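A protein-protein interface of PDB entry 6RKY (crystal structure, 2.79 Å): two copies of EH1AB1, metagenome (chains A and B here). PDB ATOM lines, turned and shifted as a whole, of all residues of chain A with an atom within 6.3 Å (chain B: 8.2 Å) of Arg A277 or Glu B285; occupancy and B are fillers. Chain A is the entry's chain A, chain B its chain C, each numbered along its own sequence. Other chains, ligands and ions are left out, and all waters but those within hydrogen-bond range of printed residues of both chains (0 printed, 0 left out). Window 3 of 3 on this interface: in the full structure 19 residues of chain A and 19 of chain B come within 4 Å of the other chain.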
ATOM      1  N   VAL A 264      -6.175  15.595   8.277  1.00  0.00           N
ATOM      2  CA  VAL A 264      -6.209  16.998   7.782  1.00  0.00           C
ATOM      3  C   VAL A 264      -7.552  17.236   7.069  1.00  0.00           C
ATOM      4  O   VAL A 264      -7.931  16.441   6.204  1.00  0.00           O
ATOM      5  CB  VAL A 264      -4.989  17.290   6.901  1.00  0.00           C
ATOM      6  CG1 VAL A 264      -4.996  18.705   6.328  1.00  0.00           C
ATOM      7  CG2 VAL A 264      -3.705  17.016   7.658  1.00  0.00           C
ATOM      8  N   THR A 266      -9.980  20.369   5.056  1.00  0.00           N
ATOM      9  CA  THR A 266     -10.019  21.689   4.391  1.00  0.00           C
ATOM     10  C   THR A 266     -11.459  21.958   3.958  1.00  0.00           C
ATOM     11  O   THR A 266     -12.203  20.999   3.799  1.00  0.00           O
ATOM     12  CB  THR A 266      -8.990  21.781   3.251  1.00  0.00           C
ATOM     13  OG1 THR A 266      -9.304  20.826   2.231  1.00  0.00           O
ATOM     14  CG2 THR A 266      -7.569  21.554   3.729  1.00  0.00           C
ATOM     15  N   LEU A 272      -7.121  29.250   3.122  1.00  0.00           N
ATOM     16  CA  LEU A 272      -6.072  28.318   3.639  1.00  0.00           C
ATOM     17  C   LEU A 272      -6.138  26.934   2.993  1.00  0.00           C
ATOM     18  O   LEU A 272      -5.259  26.098   3.347  1.00  0.00           O
ATOM     19  CB  LEU A 272      -6.233  28.211   5.160  1.00  0.00           C
ATOM     20  CG  LEU A 272      -6.094  29.520   5.932  1.00  0.00           C
ATOM     21  CD1 LEU A 272      -6.146  29.256   7.410  1.00  0.00           C
ATOM     22  CD2 LEU A 272      -4.810  30.245   5.577  1.00  0.00           C
ATOM     23  N   ARG A 273      -7.092  26.678   2.099  1.00  0.00           N
ATOM     24  CA  ARG A 273      -7.280  25.317   1.527  1.00  0.00           C
ATOM     25  C   ARG A 273      -5.958  24.769   1.015  1.00  0.00           C
ATOM     26  O   ARG A 273      -5.556  23.692   1.484  1.00  0.00           O
ATOM     27  CB  ARG A 273      -8.289  25.307   0.381  1.00  0.00           C
ATOM     28  CG  ARG A 273      -8.583  23.929  -0.195  1.00  0.00           C
ATOM     29  CD  ARG A 273      -9.467  24.163  -1.410  1.00  0.00           C
ATOM     30  NE  ARG A 273      -8.686  24.649  -2.544  1.00  0.00           N
ATOM     31  CZ  ARG A 273      -9.154  25.298  -3.608  1.00  0.00           C
ATOM     32  NH1 ARG A 273     -10.435  25.583  -3.720  1.00  0.00           N
ATOM     33  NH2 ARG A 273      -8.325  25.665  -4.568  1.00  0.00           N
ATOM     34  N   ASP A 274      -5.308  25.492   0.091  1.00  0.00           N
ATOM     35  CA  ASP A 274      -4.140  25.006  -0.691  1.00  0.00           C
ATOM     36  C   ASP A 274      -2.966  24.658   0.239  1.00  0.00           C
ATOM     37  O   ASP A 274      -2.325  23.593   0.012  1.00  0.00           O
ATOM     38  CB  ASP A 274      -3.780  26.008  -1.792  1.00  0.00           C
ATOM     39  CG  ASP A 274      -4.792  26.057  -2.938  1.00  0.00           C
ATOM     40  OD1 ASP A 274      -5.843  25.376  -2.835  1.00  0.00           O
ATOM     41  OD2 ASP A 274      -4.532  26.772  -3.935  1.00  0.00           O
ATOM     42  N   GLU A 275      -2.676  25.497   1.242  1.00  0.00           N
ATOM     43  CA  GLU A 275      -1.572  25.234   2.198  1.00  0.00           C
ATOM     44  C   GLU A 275      -1.966  24.064   3.109  1.00  0.00           C
ATOM     45  O   GLU A 275      -1.086  23.207   3.398  1.00  0.00           O
ATOM     46  CB  GLU A 275      -1.142  26.512   2.916  1.00  0.00           C
ATOM     47  CG  GLU A 275      -2.162  27.094   3.859  1.00  0.00           C
ATOM     48  CD  GLU A 275      -1.959  28.592   4.080  1.00  0.00           C
ATOM     49  OE1 GLU A 275      -2.251  29.363   3.152  1.00  0.00           O
ATOM     50  OE2 GLU A 275      -1.508  28.988   5.182  1.00  0.00           O
ATOM     51  N   GLY A 276      -3.249  23.952   3.468  1.00  0.00           N
ATOM     52  CA  GLY A 276      -3.760  22.772   4.202  1.00  0.00           C
ATOM     53  C   GLY A 276      -3.462  21.479   3.450  1.00  0.00           C
ATOM     54  O   GLY A 276      -2.956  20.509   4.053  1.00  0.00           O
ATOM     55  N   ARG A 277      -3.767  21.460   2.154  1.00  0.00           N
ATOM     56  CA  ARG A 277      -3.639  20.244   1.311  1.00  0.00           C
ATOM     57  C   ARG A 277      -2.153  19.972   1.039  1.00  0.00           C
ATOM     58  O   ARG A 277      -1.777  18.794   1.068  1.00  0.00           O
ATOM     59  CB  ARG A 277      -4.459  20.400   0.028  1.00  0.00           C
ATOM     60  CG  ARG A 277      -3.979  19.512  -1.108  1.00  0.00           C
ATOM     61  CD  ARG A 277      -5.032  19.383  -2.176  1.00  0.00           C
ATOM     62  NE  ARG A 277      -4.989  18.046  -2.749  1.00  0.00           N
ATOM     63  CZ  ARG A 277      -5.283  17.753  -4.003  1.00  0.00           C
ATOM     64  NH1 ARG A 277      -5.668  18.709  -4.831  1.00  0.00           N
ATOM     65  NH2 ARG A 277      -5.207  16.495  -4.406  1.00  0.00           N
ATOM     66  N   ALA A 278      -1.352  21.012   0.768  1.00  0.00           N
ATOM     67  CA  ALA A 278       0.116  20.908   0.597  1.00  0.00           C
ATOM     68  C   ALA A 278       0.747  20.172   1.795  1.00  0.00           C
ATOM     69  O   ALA A 278       1.498  19.200   1.572  1.00  0.00           O
ATOM     70  CB  ALA A 278       0.705  22.292   0.425  1.00  0.00           C
ATOM     71  N   TYR A 279       0.441  20.605   3.024  1.00  0.00           N
ATOM     72  CA  TYR A 279       0.933  19.971   4.277  1.00  0.00           C
ATOM     73  C   TYR A 279       0.600  18.474   4.248  1.00  0.00           C
ATOM     74  O   TYR A 279       1.512  17.648   4.476  1.00  0.00           O
ATOM     75  CB  TYR A 279       0.365  20.650   5.535  1.00  0.00           C
ATOM     76  CG  TYR A 279       1.186  20.432   6.785  1.00  0.00           C
ATOM     77  CD1 TYR A 279       2.315  21.196   7.053  1.00  0.00           C
ATOM     78  CD2 TYR A 279       0.849  19.448   7.699  1.00  0.00           C
ATOM     79  CE1 TYR A 279       3.077  21.001   8.192  1.00  0.00           C
ATOM     80  CE2 TYR A 279       1.600  19.235   8.838  1.00  0.00           C
ATOM     81  CZ  TYR A 279       2.714  20.024   9.094  1.00  0.00           C
ATOM     82  OH  TYR A 279       3.455  19.817  10.231  1.00  0.00           O
ATOM     83  N   ALA A 280      -0.664  18.129   3.992  1.00  0.00           N
ATOM     84  CA  ALA A 280      -1.134  16.730   3.839  1.00  0.00           C
ATOM     85  C   ALA A 280      -0.262  15.981   2.829  1.00  0.00           C
ATOM     86  O   ALA A 280       0.180  14.866   3.155  1.00  0.00           O
ATOM     87  CB  ALA A 280      -2.574  16.709   3.422  1.00  0.00           C
ATOM     88  N   ASP A 281      -0.014  16.567   1.656  1.00  0.00           N
ATOM     89  CA  ASP A 281       0.811  15.951   0.580  1.00  0.00           C
ATOM     90  C   ASP A 281       2.230  15.693   1.108  1.00  0.00           C
ATOM     91  O   ASP A 281       2.769  14.578   0.865  1.00  0.00           O
ATOM     92  CB  ASP A 281       0.833  16.811  -0.685  1.00  0.00           C
ATOM     93  CG  ASP A 281      -0.469  16.819  -1.477  1.00  0.00           C
ATOM     94  OD1 ASP A 281      -1.329  15.921  -1.237  1.00  0.00           O
ATOM     95  OD2 ASP A 281      -0.617  17.721  -2.339  1.00  0.00           O
ATOM     96  N   ARG A 282       2.817  16.661   1.813  1.00  0.00           N
ATOM     97  CA  ARG A 282       4.195  16.539   2.366  1.00  0.00           C
ATOM     98  C   ARG A 282       4.259  15.336   3.319  1.00  0.00           C
ATOM     99  O   ARG A 282       5.258  14.592   3.263  1.00  0.00           O
ATOM    100  CB  ARG A 282       4.621  17.838   3.057  1.00  0.00           C
ATOM    101  CG  ARG A 282       4.768  19.049   2.139  1.00  0.00           C
ATOM    102  CD  ARG A 282       5.867  18.954   1.094  1.00  0.00           C
ATOM    103  NE  ARG A 282       7.145  18.632   1.719  1.00  0.00           N
ATOM    104  CZ  ARG A 282       7.953  19.501   2.339  1.00  0.00           C
ATOM    105  NH1 ARG A 282       7.639  20.787   2.409  1.00  0.00           N
ATOM    106  NH2 ARG A 282       9.070  19.064   2.897  1.00  0.00           N
ATOM    107  N   ILE A 284       2.146  12.624   3.413  1.00  0.00           N
ATOM    108  CA  ILE A 284       1.824  11.370   2.668  1.00  0.00           C
ATOM    109  C   ILE A 284       3.098  10.849   1.988  1.00  0.00           C
ATOM    110  O   ILE A 284       3.395   9.625   2.124  1.00  0.00           O
ATOM    111  CB  ILE A 284       0.652  11.600   1.683  1.00  0.00           C
ATOM    112  CG1 ILE A 284      -0.660  11.798   2.447  1.00  0.00           C
ATOM    113  CG2 ILE A 284       0.524  10.471   0.661  1.00  0.00           C
ATOM    114  CD1 ILE A 284      -1.716  12.562   1.672  1.00  0.00           C
ATOM    115  N   TYR A 292      -6.819  12.569   4.583  1.00  0.00           N
ATOM    116  CA  TYR A 292      -7.045  13.925   4.019  1.00  0.00           C
ATOM    117  C   TYR A 292      -8.507  14.002   3.550  1.00  0.00           C
ATOM    118  O   TYR A 292      -8.951  13.095   2.787  1.00  0.00           O
ATOM    119  CB  TYR A 292      -6.033  14.290   2.908  1.00  0.00           C
ATOM    120  CG  TYR A 292      -6.406  15.600   2.281  1.00  0.00           C
ATOM    121  CD1 TYR A 292      -6.176  16.799   2.934  1.00  0.00           C
ATOM    122  CD2 TYR A 292      -7.167  15.636   1.125  1.00  0.00           C
ATOM    123  CE1 TYR A 292      -6.636  18.005   2.427  1.00  0.00           C
ATOM    124  CE2 TYR A 292      -7.635  16.834   0.601  1.00  0.00           C
ATOM    125  CZ  TYR A 292      -7.370  18.017   1.261  1.00  0.00           C
ATOM    126  OH  TYR A 292      -7.828  19.177   0.731  1.00  0.00           O
ATOM    127  N   PHE B 256     -15.591  14.127 -13.866  1.00  0.00           N
ATOM    128  CA  PHE B 256     -15.780  13.528 -12.517  1.00  0.00           C
ATOM    129  C   PHE B 256     -16.886  14.244 -11.731  1.00  0.00           C
ATOM    130  O   PHE B 256     -17.184  13.806 -10.599  1.00  0.00           O
ATOM    131  CB  PHE B 256     -14.470  13.541 -11.727  1.00  0.00           C
ATOM    132  CG  PHE B 256     -13.599  12.344 -11.991  1.00  0.00           C
ATOM    133  CD1 PHE B 256     -12.946  12.202 -13.211  1.00  0.00           C
ATOM    134  CD2 PHE B 256     -13.433  11.363 -11.031  1.00  0.00           C
ATOM    135  CE1 PHE B 256     -12.134  11.108 -13.458  1.00  0.00           C
ATOM    136  CE2 PHE B 256     -12.632  10.256 -11.283  1.00  0.00           C
ATOM    137  CZ  PHE B 256     -11.988  10.129 -12.496  1.00  0.00           C
ATOM    138  N   THR B 257     -17.505  15.278 -12.294  1.00  0.00           N
ATOM    139  CA  THR B 257     -18.630  15.999 -11.632  1.00  0.00           C
ATOM    140  C   THR B 257     -19.830  15.046 -11.574  1.00  0.00           C
ATOM    141  O   THR B 257     -19.940  14.188 -12.470  1.00  0.00           O
ATOM    142  CB  THR B 257     -18.939  17.350 -12.301  1.00  0.00           C
ATOM    143  OG1 THR B 257     -19.436  17.093 -13.610  1.00  0.00           O
ATOM    144  CG2 THR B 257     -17.744  18.285 -12.377  1.00  0.00           C
ATOM    145  N   ARG B 277      -4.593   6.778  -5.659  1.00  0.00           N
ATOM    146  CA  ARG B 277      -4.433   8.180  -5.207  1.00  0.00           C
ATOM    147  C   ARG B 277      -4.815   9.132  -6.345  1.00  0.00           C
ATOM    148  O   ARG B 277      -5.459  10.138  -6.060  1.00  0.00           O
ATOM    149  CB  ARG B 277      -3.009   8.404  -4.698  1.00  0.00           C
ATOM    150  CG  ARG B 277      -2.632   9.869  -4.654  1.00  0.00           C
ATOM    151  CD  ARG B 277      -1.394  10.063  -3.838  1.00  0.00           C
ATOM    152  NE  ARG B 277      -1.399  11.397  -3.289  1.00  0.00           N
ATOM    153  CZ  ARG B 277      -0.336  11.994  -2.798  1.00  0.00           C
ATOM    154  NH1 ARG B 277       0.819  11.356  -2.791  1.00  0.00           N
ATOM    155  NH2 ARG B 277      -0.433  13.228  -2.319  1.00  0.00           N
ATOM    156  N   ALA B 278      -4.421   8.832  -7.589  1.00  0.00           N
ATOM    157  CA  ALA B 278      -4.813   9.595  -8.800  1.00  0.00           C
ATOM    158  C   ALA B 278      -6.344   9.763  -8.854  1.00  0.00           C
ATOM    159  O   ALA B 278      -6.804  10.919  -9.006  1.00  0.00           O
ATOM    160  CB  ALA B 278      -4.281   8.905 -10.025  1.00  0.00           C
ATOM    161  N   TYR B 279      -7.107   8.670  -8.713  1.00  0.00           N
ATOM    162  CA  TYR B 279      -8.595   8.700  -8.717  1.00  0.00           C
ATOM    163  C   TYR B 279      -9.091   9.687  -7.650  1.00  0.00           C
ATOM    164  O   TYR B 279      -9.916  10.557  -7.957  1.00  0.00           O
ATOM    165  CB  TYR B 279      -9.197   7.307  -8.501  1.00  0.00           C
ATOM    166  CG  TYR B 279     -10.622   7.147  -8.986  1.00  0.00           C
ATOM    167  CD1 TYR B 279     -10.906   6.896 -10.313  1.00  0.00           C
ATOM    168  CD2 TYR B 279     -11.690   7.251  -8.119  1.00  0.00           C
ATOM    169  CE1 TYR B 279     -12.212   6.763 -10.772  1.00  0.00           C
ATOM    170  CE2 TYR B 279     -13.001   7.114  -8.552  1.00  0.00           C
ATOM    171  CZ  TYR B 279     -13.268   6.867  -9.887  1.00  0.00           C
ATOM    172  OH  TYR B 279     -14.555   6.732 -10.324  1.00  0.00           O
ATOM    173  N   ALA B 280      -8.590   9.562  -6.420  1.00  0.00           N
ATOM    174  CA  ALA B 280      -8.879  10.494  -5.301  1.00  0.00           C
ATOM    175  C   ALA B 280      -8.611  11.940  -5.735  1.00  0.00           C
ATOM    176  O   ALA B 280      -9.484  12.787  -5.503  1.00  0.00           O
ATOM    177  CB  ALA B 280      -8.055  10.126  -4.095  1.00  0.00           C
ATOM    178  N   ASP B 281      -7.453  12.212  -6.338  1.00  0.00           N
ATOM    179  CA  ASP B 281      -7.064  13.573  -6.800  1.00  0.00           C
ATOM    180  C   ASP B 281      -8.090  14.077  -7.819  1.00  0.00           C
ATOM    181  O   ASP B 281      -8.512  15.261  -7.715  1.00  0.00           O
ATOM    182  CB  ASP B 281      -5.643  13.609  -7.372  1.00  0.00           C
ATOM    183  CG  ASP B 281      -4.519  13.462  -6.346  1.00  0.00           C
ATOM    184  OD1 ASP B 281      -4.784  13.624  -5.108  1.00  0.00           O
ATOM    185  OD2 ASP B 281      -3.374  13.172  -6.787  1.00  0.00           O
ATOM    186  N   ARG B 282      -8.492  13.230  -8.763  1.00  0.00           N
ATOM    187  CA  ARG B 282      -9.474  13.598  -9.821  1.00  0.00           C
ATOM    188  C   ARG B 282     -10.796  14.024  -9.175  1.00  0.00           C
ATOM    189  O   ARG B 282     -11.389  15.017  -9.647  1.00  0.00           O
ATOM    190  CB  ARG B 282      -9.664  12.446 -10.813  1.00  0.00           C
ATOM    191  CG  ARG B 282      -8.430  12.111 -11.646  1.00  0.00           C
ATOM    192  CD  ARG B 282      -7.988  13.210 -12.602  1.00  0.00           C
ATOM    193  NE  ARG B 282      -9.082  13.657 -13.461  1.00  0.00           N
ATOM    194  CZ  ARG B 282      -9.510  13.026 -14.559  1.00  0.00           C
ATOM    195  NH1 ARG B 282      -8.926  11.907 -14.971  1.00  0.00           N
ATOM    196  NH2 ARG B 282     -10.531  13.524 -15.242  1.00  0.00           N
ATOM    197  N   LEU B 283     -11.243  13.310  -8.135  1.00  0.00           N
ATOM    198  CA  LEU B 283     -12.522  13.594  -7.427  1.00  0.00           C
ATOM    199  C   LEU B 283     -12.406  14.925  -6.670  1.00  0.00           C
ATOM    200  O   LEU B 283     -13.348  15.726  -6.741  1.00  0.00           O
ATOM    201  CB  LEU B 283     -12.874  12.439  -6.480  1.00  0.00           C
ATOM    202  CG  LEU B 283     -13.395  11.146  -7.120  1.00  0.00           C
ATOM    203  CD1 LEU B 283     -13.255   9.973  -6.177  1.00  0.00           C
ATOM    204  CD2 LEU B 283     -14.844  11.280  -7.519  1.00  0.00           C
ATOM    205  N   ILE B 284     -11.292  15.141  -5.971  1.00  0.00           N
ATOM    206  CA  ILE B 284     -11.053  16.347  -5.121  1.00  0.00           C
ATOM    207  C   ILE B 284     -11.091  17.615  -5.994  1.00  0.00           C
ATOM    208  O   ILE B 284     -11.794  18.594  -5.606  1.00  0.00           O
ATOM    209  CB  ILE B 284      -9.748  16.196  -4.309  1.00  0.00           C
ATOM    210  CG1 ILE B 284      -9.885  15.083  -3.263  1.00  0.00           C
ATOM    211  CG2 ILE B 284      -9.356  17.507  -3.655  1.00  0.00           C
ATOM    212  CD1 ILE B 284      -8.565  14.495  -2.797  1.00  0.00           C
ATOM    213  N   GLU B 285     -10.415  17.575  -7.145  1.00  0.00           N
ATOM    214  CA  GLU B 285     -10.296  18.716  -8.100  1.00  0.00           C
ATOM    215  C   GLU B 285     -11.644  18.990  -8.781  1.00  0.00           C
ATOM    216  O   GLU B 285     -11.863  20.121  -9.172  1.00  0.00           O
ATOM    217  CB  GLU B 285      -9.144  18.448  -9.086  1.00  0.00           C
ATOM    218  CG  GLU B 285      -7.776  18.857  -8.536  1.00  0.00           C
ATOM    219  CD  GLU B 285      -6.654  17.822  -8.540  1.00  0.00           C
ATOM    220  OE1 GLU B 285      -6.702  16.890  -9.373  1.00  0.00           O
ATOM    221  OE2 GLU B 285      -5.713  17.961  -7.712  1.00  0.00           O
ATOM    222  N   ALA B 286     -12.525  17.998  -8.889  1.00  0.00           N
ATOM    223  CA  ALA B 286     -13.884  18.139  -9.464  1.00  0.00           C
ATOM    224  C   ALA B 286     -14.906  18.679  -8.437  1.00  0.00           C
ATOM    225  O   ALA B 286     -16.067  18.895  -8.836  1.00  0.00           O
ATOM    226  CB  ALA B 286     -14.325  16.796  -9.995  1.00  0.00           C
ATOM    227  N   GLY B 287     -14.527  18.853  -7.167  1.00  0.00           N
ATOM    228  CA  GLY B 287     -15.409  19.408  -6.125  1.00  0.00           C
ATOM    229  C   GLY B 287     -16.351  18.368  -5.512  1.00  0.00           C
ATOM    230  O   GLY B 287     -17.436  18.753  -5.019  1.00  0.00           O
ATOM    231  N   ILE B 288     -15.959  17.099  -5.535  1.00  0.00           N
ATOM    232  CA  ILE B 288     -16.637  15.988  -4.801  1.00  0.00           C
ATOM    233  C   ILE B 288     -16.050  15.941  -3.380  1.00  0.00           C
ATOM    234  O   ILE B 288     -14.816  15.911  -3.273  1.00  0.00           O
ATOM    235  CB  ILE B 288     -16.466  14.630  -5.530  1.00  0.00           C
ATOM    236  CG1 ILE B 288     -16.711  14.716  -7.031  1.00  0.00           C
ATOM    237  CG2 ILE B 288     -17.341  13.550  -4.894  1.00  0.00           C
ATOM    238  CD1 ILE B 288     -18.028  15.343  -7.403  1.00  0.00           C
ATOM    239  N   THR B 290     -14.564  14.238  -0.377  1.00  0.00           N
ATOM    240  CA  THR B 290     -13.633  13.109  -0.620  1.00  0.00           C
ATOM    241  C   THR B 290     -12.698  12.976   0.577  1.00  0.00           C
ATOM    242  O   THR B 290     -12.020  13.939   0.909  1.00  0.00           O
ATOM    243  CB  THR B 290     -12.783  13.316  -1.889  1.00  0.00           C
ATOM    244  OG1 THR B 290     -13.584  13.816  -2.959  1.00  0.00           O
ATOM    245  CG2 THR B 290     -12.075  12.053  -2.348  1.00  0.00           C
ATOM    246  N   TYR B 292      -9.314  10.852   1.651  1.00  0.00           N
ATOM    247  CA  TYR B 292      -8.194  10.033   1.143  1.00  0.00           C
ATOM    248  C   TYR B 292      -7.327   9.605   2.337  1.00  0.00           C
ATOM    249  O   TYR B 292      -6.961  10.449   3.183  1.00  0.00           O
ATOM    250  CB  TYR B 292      -7.410  10.788   0.064  1.00  0.00           C
ATOM    251  CG  TYR B 292      -6.193  10.004  -0.332  1.00  0.00           C
ATOM    252  CD1 TYR B 292      -6.318   8.890  -1.146  1.00  0.00           C
ATOM    253  CD2 TYR B 292      -4.961  10.257   0.261  1.00  0.00           C
ATOM    254  CE1 TYR B 292      -5.237   8.065  -1.400  1.00  0.00           C
ATOM    255  CE2 TYR B 292      -3.865   9.454  -0.004  1.00  0.00           C
ATOM    256  CZ  TYR B 292      -4.002   8.354  -0.840  1.00  0.00           C
ATOM    257  OH  TYR B 292      -2.933   7.553  -1.112  1.00  0.00           O
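Of the 15 printed residues of chain A, 4 touch a printed residue of chain B. Printed residues of chain B that touch a printed residue of chain A: Arg B277, Asp B281, Glu B285, Thr B290 and Tyr B292. Among the printed residues, 6 pairs touch across the chains.
Arg A277 touches Asp B281, and with the chains exchanged Asp A281 touches Arg B277. Ile A284 touches Arg B277, but with the chains exchanged Arg A277 does not touch Ile B284 (4.1 Å). Tyr A292 touches its own counterpart, Tyr B292. Of the 6 pairs that touch across the chains among the printed residues, 3 have their exchanged pair printed and touching as well.
OG1 of Thr A266 lies within hydrogen-bond range of OH of Tyr A292 (2.7 Å). The backbone carbonyl oxygen (O) of Ile B288 lies within hydrogen-bond range of the side-chain hydroxyl (OG1) of Thr B290 (2.5 Å).
CG2 of Ile A284 touches NH1 of Arg B277, at 3.6 Å. Tyr A292 touches Thr B290.
No residue of chain B comes within 4 Å of Gly A276. Arg A277 touches two residues of chain B. No residue of chain B comes within 4 Å of Ala A278. Of the printed residues of chain B, Asp A281 touches Arg B277. Printed residues of chain B within 4 Å of Ile A284: Arg B277. Of the printed residues of chain A, Asp B281 touches Arg A277 (3.0 Å). Leu B283 touches none of the printed residues of chain A. Glu B285 touches one residue of chain A. Ala B286 touches none of the printed residues of chain A. The nearest residue of chain B that does not touch Arg A277 is Ile B284 (4.1 Å). The nearest printed residue of chain A that does not touch Glu B285 is Asp A281 (7.4 Å). The nearest printed residue of chain A that does not touch Tyr B292 is Ile A284 (4.1 Å).
The guanidinium group (NH2) of Arg A277 is in salt-bridge range of the side-chain carboxylate (OD1) of Asp B281 (3.0 Å). OE2 of Glu B285 lies within salt-bridge range of NH1 of Arg A277. OD1 of Asp A281 lies within salt-bridge range of NH2 of Arg B277. The backbone carbonyl oxygen (O) of Tyr A292 is in hydrogen-bond range of the backbone NH (N) of Tyr B292 (2.5 Å).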
